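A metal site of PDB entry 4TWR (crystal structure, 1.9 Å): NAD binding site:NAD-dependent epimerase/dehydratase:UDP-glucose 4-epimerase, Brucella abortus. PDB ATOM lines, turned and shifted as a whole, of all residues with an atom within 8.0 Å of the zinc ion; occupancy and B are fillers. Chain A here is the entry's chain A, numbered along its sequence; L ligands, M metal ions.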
ATOM      1  N   PHE A  22      27.108  21.254 -24.169  1.00  0.00           N
ATOM      2  CA  PHE A  22      27.480  22.404 -23.337  1.00  0.00           C
ATOM      3  C   PHE A  22      28.824  22.186 -22.639  1.00  0.00           C
ATOM      4  O   PHE A  22      29.823  22.854 -22.948  1.00  0.00           O
ATOM      5  CB  PHE A  22      26.360  22.663 -22.315  1.00  0.00           C
ATOM      6  CG  PHE A  22      26.606  23.835 -21.400  1.00  0.00           C
ATOM      7  CD1 PHE A  22      27.308  24.956 -21.841  1.00  0.00           C
ATOM      8  CD2 PHE A  22      26.144  23.824 -20.093  1.00  0.00           C
ATOM      9  CE1 PHE A  22      27.538  26.033 -20.988  1.00  0.00           C
ATOM     10  CE2 PHE A  22      26.354  24.902 -19.239  1.00  0.00           C
ATOM     11  CZ  PHE A  22      27.055  26.002 -19.686  1.00  0.00           C
ATOM     12  N   ALA A  87      19.792  15.172 -20.637  1.00  0.00           N
ATOM     13  CA  ALA A  87      18.905  15.155 -19.476  1.00  0.00           C
ATOM     14  C   ALA A  87      18.128  16.433 -19.401  1.00  0.00           C
ATOM     15  O   ALA A  87      18.688  17.519 -19.543  1.00  0.00           O
ATOM     16  CB  ALA A  87      19.697  14.945 -18.186  1.00  0.00           C
ATOM     17  N   TYR A  88      16.828  16.298 -19.180  1.00  0.00           N
ATOM     18  CA  TYR A  88      16.021  17.451 -18.926  1.00  0.00           C
ATOM     19  C   TYR A  88      15.529  17.324 -17.491  1.00  0.00           C
ATOM     20  O   TYR A  88      15.299  16.220 -16.990  1.00  0.00           O
ATOM     21  CB  TYR A  88      14.863  17.560 -19.925  1.00  0.00           C
ATOM     22  CG  TYR A  88      15.343  17.644 -21.370  1.00  0.00           C
ATOM     23  CD1 TYR A  88      15.786  18.846 -21.909  1.00  0.00           C
ATOM     24  CD2 TYR A  88      15.353  16.514 -22.191  1.00  0.00           C
ATOM     25  CE1 TYR A  88      16.230  18.928 -23.220  1.00  0.00           C
ATOM     26  CE2 TYR A  88      15.786  16.577 -23.498  1.00  0.00           C
ATOM     27  CZ  TYR A  88      16.230  17.785 -24.008  1.00  0.00           C
ATOM     28  OH  TYR A  88      16.654  17.868 -25.318  1.00  0.00           O
ATOM     29  N   VAL A  89      15.445  18.476 -16.825  1.00  0.00           N
ATOM     30  CA  VAL A  89      15.030  18.544 -15.424  1.00  0.00           C
ATOM     31  C   VAL A  89      13.595  18.087 -15.254  1.00  0.00           C
ATOM     32  O   VAL A  89      12.691  18.687 -15.812  1.00  0.00           O
ATOM     33  CB  VAL A  89      15.184  19.978 -14.886  1.00  0.00           C
ATOM     34  CG1 VAL A  89      14.580  20.091 -13.496  1.00  0.00           C
ATOM     35  CG2 VAL A  89      16.672  20.393 -14.906  1.00  0.00           C
ATOM     36  N   ALA A 181      25.703  23.037 -13.826  1.00  0.00           N
ATOM     37  CA  ALA A 181      26.623  23.707 -14.735  1.00  0.00           C
ATOM     38  C   ALA A 181      26.044  25.053 -15.141  1.00  0.00           C
ATOM     39  O   ALA A 181      24.875  25.129 -15.510  1.00  0.00           O
ATOM     40  CB  ALA A 181      26.872  22.864 -15.960  1.00  0.00           C
ATOM     41  N   GLU A 192      25.508  27.705 -23.765  1.00  0.00           N
ATOM     42  CA  GLU A 192      24.601  26.611 -23.475  1.00  0.00           C
ATOM     43  C   GLU A 192      23.394  26.673 -24.411  1.00  0.00           C
ATOM     44  O   GLU A 192      22.572  27.570 -24.308  1.00  0.00           O
ATOM     45  CB  GLU A 192      24.149  26.695 -22.004  1.00  0.00           C
ATOM     46  CG  GLU A 192      23.052  25.727 -21.579  1.00  0.00           C
ATOM     47  CD  GLU A 192      22.839  25.768 -20.077  1.00  0.00           C
ATOM     48  OE1 GLU A 192      23.376  26.683 -19.417  1.00  0.00           O
ATOM     49  OE2 GLU A 192      22.128  24.889 -19.553  1.00  0.00           O
ATOM     50  N   LYS A 193      23.297  25.720 -25.336  1.00  0.00           N
ATOM     51  CA  LYS A 193      22.206  25.728 -26.317  1.00  0.00           C
ATOM     52  C   LYS A 193      21.369  24.461 -26.157  1.00  0.00           C
ATOM     53  O   LYS A 193      21.690  23.410 -26.741  1.00  0.00           O
ATOM     54  CB  LYS A 193      22.758  25.835 -27.739  1.00  0.00           C
ATOM     55  N   HIS A 194      20.306  24.577 -25.374  1.00  0.00           N
ATOM     56  CA  HIS A 194      19.430  23.454 -25.069  1.00  0.00           C
ATOM     57  C   HIS A 194      18.027  23.784 -25.532  1.00  0.00           C
ATOM     58  O   HIS A 194      17.624  24.949 -25.500  1.00  0.00           O
ATOM     59  CB  HIS A 194      19.453  23.160 -23.569  1.00  0.00           C
ATOM     60  CG  HIS A 194      20.759  22.626 -23.071  1.00  0.00           C
ATOM     61  ND1 HIS A 194      21.185  22.768 -21.768  1.00  0.00           N
ATOM     62  CD2 HIS A 194      21.732  21.912 -23.698  1.00  0.00           C
ATOM     63  CE1 HIS A 194      22.357  22.188 -21.613  1.00  0.00           C
ATOM     64  NE2 HIS A 194      22.711  21.660 -22.775  1.00  0.00           N
ATOM     65  N   ASP A 195      17.292  22.779 -25.971  1.00  0.00           N
ATOM     66  CA  ASP A 195      15.934  22.981 -26.451  1.00  0.00           C
ATOM     67  C   ASP A 195      15.177  21.678 -26.256  1.00  0.00           C
ATOM     68  O   ASP A 195      15.376  20.722 -26.998  1.00  0.00           O
ATOM     69  CB  ASP A 195      15.947  23.425 -27.911  1.00  0.00           C
ATOM     70  CG  ASP A 195      14.561  23.729 -28.451  1.00  0.00           C
ATOM     71  OD1 ASP A 195      13.595  23.760 -27.664  1.00  0.00           O
ATOM     72  OD2 ASP A 195      14.453  23.940 -29.675  1.00  0.00           O
ATOM     73  N   PRO A 196      14.304  21.623 -25.231  1.00  0.00           N
ATOM     74  CA  PRO A 196      13.986  22.703 -24.306  1.00  0.00           C
ATOM     75  C   PRO A 196      15.099  23.002 -23.317  1.00  0.00           C
ATOM     76  O   PRO A 196      15.866  22.116 -22.930  1.00  0.00           O
ATOM     77  CB  PRO A 196      12.755  22.182 -23.569  1.00  0.00           C
ATOM     78  CG  PRO A 196      12.978  20.731 -23.536  1.00  0.00           C
ATOM     79  CD  PRO A 196      13.545  20.401 -24.890  1.00  0.00           C
ATOM     80  N   GLU A 197      15.182  24.265 -22.926  1.00  0.00           N
ATOM     81  CA  GLU A 197      16.121  24.707 -21.919  1.00  0.00           C
ATOM     82  C   GLU A 197      15.487  24.562 -20.547  1.00  0.00           C
ATOM     83  O   GLU A 197      14.523  25.254 -20.222  1.00  0.00           O
ATOM     84  CB  GLU A 197      16.533  26.153 -22.170  1.00  0.00           C
ATOM     85  CG  GLU A 197      17.468  26.705 -21.124  1.00  0.00           C
ATOM     86  CD  GLU A 197      18.759  25.900 -21.050  1.00  0.00           C
ATOM     87  OE1 GLU A 197      19.643  26.111 -21.914  1.00  0.00           O
ATOM     88  OE2 GLU A 197      18.883  25.053 -20.135  1.00  0.00           O
ATOM     89  N   THR A 198      16.026  23.670 -19.731  1.00  0.00           N
ATOM     90  CA  THR A 198      15.382  23.362 -18.458  1.00  0.00           C
ATOM     91  C   THR A 198      16.197  23.798 -17.251  1.00  0.00           C
ATOM     92  O   THR A 198      15.755  23.650 -16.110  1.00  0.00           O
ATOM     93  CB  THR A 198      15.084  21.849 -18.361  1.00  0.00           C
ATOM     94  OG1 THR A 198      16.316  21.113 -18.360  1.00  0.00           O
ATOM     95  CG2 THR A 198      14.248  21.389 -19.542  1.00  0.00           C
ATOM     96  N   HIS A 199      17.383  24.342 -17.490  1.00  0.00           N
ATOM     97  CA  HIS A 199      18.245  24.775 -16.386  1.00  0.00           C
ATOM     98  C   HIS A 199      17.895  26.170 -15.923  1.00  0.00           C
ATOM     99  O   HIS A 199      17.505  27.021 -16.716  1.00  0.00           O
ATOM    100  CB  HIS A 199      19.711  24.682 -16.792  1.00  0.00           C
ATOM    101  CG  HIS A 199      20.114  23.292 -17.176  1.00  0.00           C
ATOM    102  ND1 HIS A 199      20.289  22.904 -18.482  1.00  0.00           N
ATOM    103  CD2 HIS A 199      20.272  22.173 -16.432  1.00  0.00           C
ATOM    104  CE1 HIS A 199      20.586  21.618 -18.526  1.00  0.00           C
ATOM    105  NE2 HIS A 199      20.575  21.147 -17.296  1.00  0.00           N
ATOM    106  N   LEU A 200      18.033  26.382 -14.623  1.00  0.00           N
ATOM    107  CA  LEU A 200      17.419  27.522 -13.955  1.00  0.00           C
ATOM    108  C   LEU A 200      17.929  28.866 -14.434  1.00  0.00           C
ATOM    109  O   LEU A 200      17.152  29.737 -14.797  1.00  0.00           O
ATOM    110  CB  LEU A 200      17.610  27.417 -12.449  1.00  0.00           C
ATOM    111  CG  LEU A 200      16.918  28.570 -11.729  1.00  0.00           C
ATOM    112  CD1 LEU A 200      15.407  28.393 -11.798  1.00  0.00           C
ATOM    113  CD2 LEU A 200      17.396  28.693 -10.312  1.00  0.00           C
ATOM    114  N   ILE A 201      19.247  29.037 -14.428  1.00  0.00           N
ATOM    115  CA  ILE A 201      19.800  30.346 -14.779  1.00  0.00           C
ATOM    116  C   ILE A 201      19.510  30.718 -16.244  1.00  0.00           C
ATOM    117  O   ILE A 201      19.127  31.868 -16.526  1.00  0.00           O
ATOM    118  CB  ILE A 201      21.303  30.407 -14.482  1.00  0.00           C
ATOM    119  CG1 ILE A 201      21.523  30.231 -12.973  1.00  0.00           C
ATOM    120  CG2 ILE A 201      21.882  31.708 -14.965  1.00  0.00           C
ATOM    121  CD1 ILE A 201      22.920  30.521 -12.525  1.00  0.00           C
ATOM    122  N   PRO A 202      19.663  29.764 -17.178  1.00  0.00           N
ATOM    123  CA  PRO A 202      19.194  30.073 -18.530  1.00  0.00           C
ATOM    124  C   PRO A 202      17.724  30.431 -18.619  1.00  0.00           C
ATOM    125  O   PRO A 202      17.367  31.338 -19.383  1.00  0.00           O
ATOM    126  CB  PRO A 202      19.469  28.773 -19.286  1.00  0.00           C
ATOM    127  CG  PRO A 202      20.690  28.255 -18.624  1.00  0.00           C
ATOM    128  CD  PRO A 202      20.485  28.531 -17.171  1.00  0.00           C
ATOM    129  N   ARG A 203      16.877  29.734 -17.881  1.00  0.00           N
ATOM    130  CA  ARG A 203      15.436  30.013 -17.903  1.00  0.00           C
ATOM    131  C   ARG A 203      15.179  31.412 -17.352  1.00  0.00           C
ATOM    132  O   ARG A 203      14.411  32.180 -17.919  1.00  0.00           O
ATOM    133  CB  ARG A 203      14.657  28.965 -17.117  1.00  0.00           C
ATOM    134  CG  ARG A 203      14.540  27.613 -17.846  1.00  0.00           C
ATOM    135  CD  ARG A 203      13.733  26.601 -17.045  1.00  0.00           C
ATOM    136  NE  ARG A 203      12.401  27.094 -16.707  1.00  0.00           N
ATOM    137  CZ  ARG A 203      11.966  27.264 -15.458  1.00  0.00           C
ATOM    138  NH1 ARG A 203      12.756  26.970 -14.427  1.00  0.00           N
ATOM    139  NH2 ARG A 203      10.730  27.731 -15.230  1.00  0.00           N
ATOM    140  N   MET A 206      16.321  33.908 -19.972  1.00  0.00           N
ATOM    141  CA  MET A 206      15.376  33.896 -21.077  1.00  0.00           C
ATOM    142  C   MET A 206      14.105  34.673 -20.737  1.00  0.00           C
ATOM    143  O   MET A 206      13.536  35.352 -21.600  1.00  0.00           O
ATOM    144  CB  MET A 206      15.016  32.460 -21.463  1.00  0.00           C
ATOM    145  CG  MET A 206      16.125  31.743 -22.227  1.00  0.00           C
ATOM    146  SD  MET A 206      15.768  29.990 -22.416  1.00  0.00           S
ATOM    147  CE  MET A 206      16.933  29.543 -23.697  1.00  0.00           C
ATOM    148  N   PHE A 330      21.756  34.673 -23.986  1.00  0.00           N
ATOM    149  CA  PHE A 330      20.306  34.573 -23.817  1.00  0.00           C
ATOM    150  C   PHE A 330      19.630  35.910 -24.085  1.00  0.00           C
ATOM    151  O   PHE A 330      18.545  36.164 -23.575  1.00  0.00           O
ATOM    152  CB  PHE A 330      19.968  34.067 -22.413  1.00  0.00           C
ATOM    153  CG  PHE A 330      20.440  32.672 -22.166  1.00  0.00           C
ATOM    154  CD1 PHE A 330      19.788  31.595 -22.737  1.00  0.00           C
ATOM    155  CD2 PHE A 330      21.556  32.440 -21.375  1.00  0.00           C
ATOM    156  CE1 PHE A 330      20.253  30.294 -22.529  1.00  0.00           C
ATOM    157  CE2 PHE A 330      22.011  31.151 -21.159  1.00  0.00           C
ATOM    158  CZ  PHE A 330      21.360  30.084 -21.732  1.00  0.00           C
HETATM  159  P1  LIG L   1      24.335  18.576 -23.247  1.00  0.00           P
HETATM  160  O1  LIG L   1      23.100  17.791 -23.641  1.00  0.00           O
HETATM  161  O2  LIG L   1      24.695  19.938 -23.765  1.00  0.00           O
HETATM  162  O3  LIG L   1      25.639  17.605 -23.875  1.00  0.00           O
HETATM  163  C1  LIG L   1      25.280  16.247 -23.981  1.00  0.00           C
HETATM  164  C2  LIG L   1      25.991  15.716 -25.248  1.00  0.00           C
HETATM  165  O4  LIG L   1      25.941  14.263 -25.316  1.00  0.00           O
HETATM  166  C3  LIG L   1      25.208  16.298 -26.420  1.00  0.00           C
HETATM  167  O5  LIG L   1      26.154  16.820 -27.299  1.00  0.00           O
HETATM  168  C4  LIG L   1      24.480  15.050 -26.994  1.00  0.00           C
HETATM  169  O6  LIG L   1      24.331  15.165 -28.391  1.00  0.00           O
HETATM  170  C5  LIG L   1      25.526  13.911 -26.648  1.00  0.00           C
HETATM  171  N1  LIG L   1      24.876  12.575 -26.492  1.00  0.00           N
HETATM  172  C6  LIG L   1      23.732  12.208 -25.739  1.00  0.00           C
HETATM  173  N2  LIG L   1      23.447  10.911 -25.830  1.00  0.00           N
HETATM  174  C7  LIG L   1      24.442  10.395 -26.682  1.00  0.00           C
HETATM  175  C8  LIG L   1      24.694   9.079 -27.178  1.00  0.00           C
HETATM  176  N3  LIG L   1      23.871   8.023 -26.838  1.00  0.00           N
HETATM  177  N4  LIG L   1      25.732   8.856 -27.990  1.00  0.00           N
HETATM  178  C9  LIG L   1      26.516   9.925 -28.321  1.00  0.00           C
HETATM  179  N5  LIG L   1      26.420  11.233 -27.942  1.00  0.00           N
HETATM  180  C10 LIG L   1      25.342  11.422 -27.101  1.00  0.00           C
HETATM  181  O7  LIG L   1      24.310  18.274 -21.693  1.00  0.00           O
HETATM  182  P2  LIG L   1      25.464  18.869 -20.746  1.00  0.00           P
HETATM  183  O8  LIG L   1      25.041  19.234 -19.344  1.00  0.00           O
HETATM  184  O9  LIG L   1      26.453  19.505 -21.661  1.00  0.00           O
HETATM  185  O10 LIG L   1      26.463  17.532 -20.378  1.00  0.00           O
HETATM  186  C11 LIG L   1      25.759  16.555 -19.834  1.00  0.00           C
HETATM  187  C12 LIG L   1      26.761  15.748 -19.074  1.00  0.00           C
HETATM  188  O11 LIG L   1      27.119  16.580 -17.951  1.00  0.00           O
HETATM  189  C13 LIG L   1      26.085  14.459 -18.549  1.00  0.00           C
HETATM  190  O12 LIG L   1      27.102  13.520 -18.426  1.00  0.00           O
HETATM  191  C14 LIG L   1      25.613  14.873 -17.165  1.00  0.00           C
HETATM  192  O13 LIG L   1      25.782  13.861 -16.198  1.00  0.00           O
HETATM  193  C15 LIG L   1      26.707  15.921 -16.809  1.00  0.00           C
HETATM  194  N6  LIG L   1      26.015  16.901 -15.839  1.00  0.00           N
HETATM  195  C16 LIG L   1      25.528  18.101 -16.342  1.00  0.00           C
HETATM  196  C17 LIG L   1      24.900  18.977 -15.414  1.00  0.00           C
HETATM  197  C18 LIG L   1      24.367  20.277 -15.885  1.00  0.00           C
HETATM  198  O14 LIG L   1      23.914  21.086 -15.063  1.00  0.00           O
HETATM  199  N7  LIG L   1      24.378  20.559 -17.240  1.00  0.00           N
HETATM  200  C19 LIG L   1      24.786  18.605 -14.067  1.00  0.00           C
HETATM  201  C20 LIG L   1      25.282  17.397 -13.603  1.00  0.00           C
HETATM  202  C21 LIG L   1      25.901  16.534 -14.513  1.00  0.00           C
HETATM  203 ZN    ZN M   1      20.487  23.885 -20.182  1.00  0.00          ZN
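The zinc ion is bound by ND1 of His 199 (2.0 Å), OE2 of Glu 197 (2.0 Å), OE2 of Glu 192 (2.0 Å) and ND1 of His 194 (2.1 Å).
The backbone NH (N) of Ala 181 is in hydrogen-bond range of an oxygen (O14) of the ligand, 2.9 Å away.
N of Phe 22 lies within hydrogen-bond range of O2 of the ligand (2.8 Å).
NE2 of His 194 is in hydrogen-bond range of O2 of the ligand.
Within 4 Å of the zinc ion: Glu 192, His 194, Glu 197 and His 199.
The nearest printed residue that does not touch the zinc ion is Thr 198 (4.5 Å).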
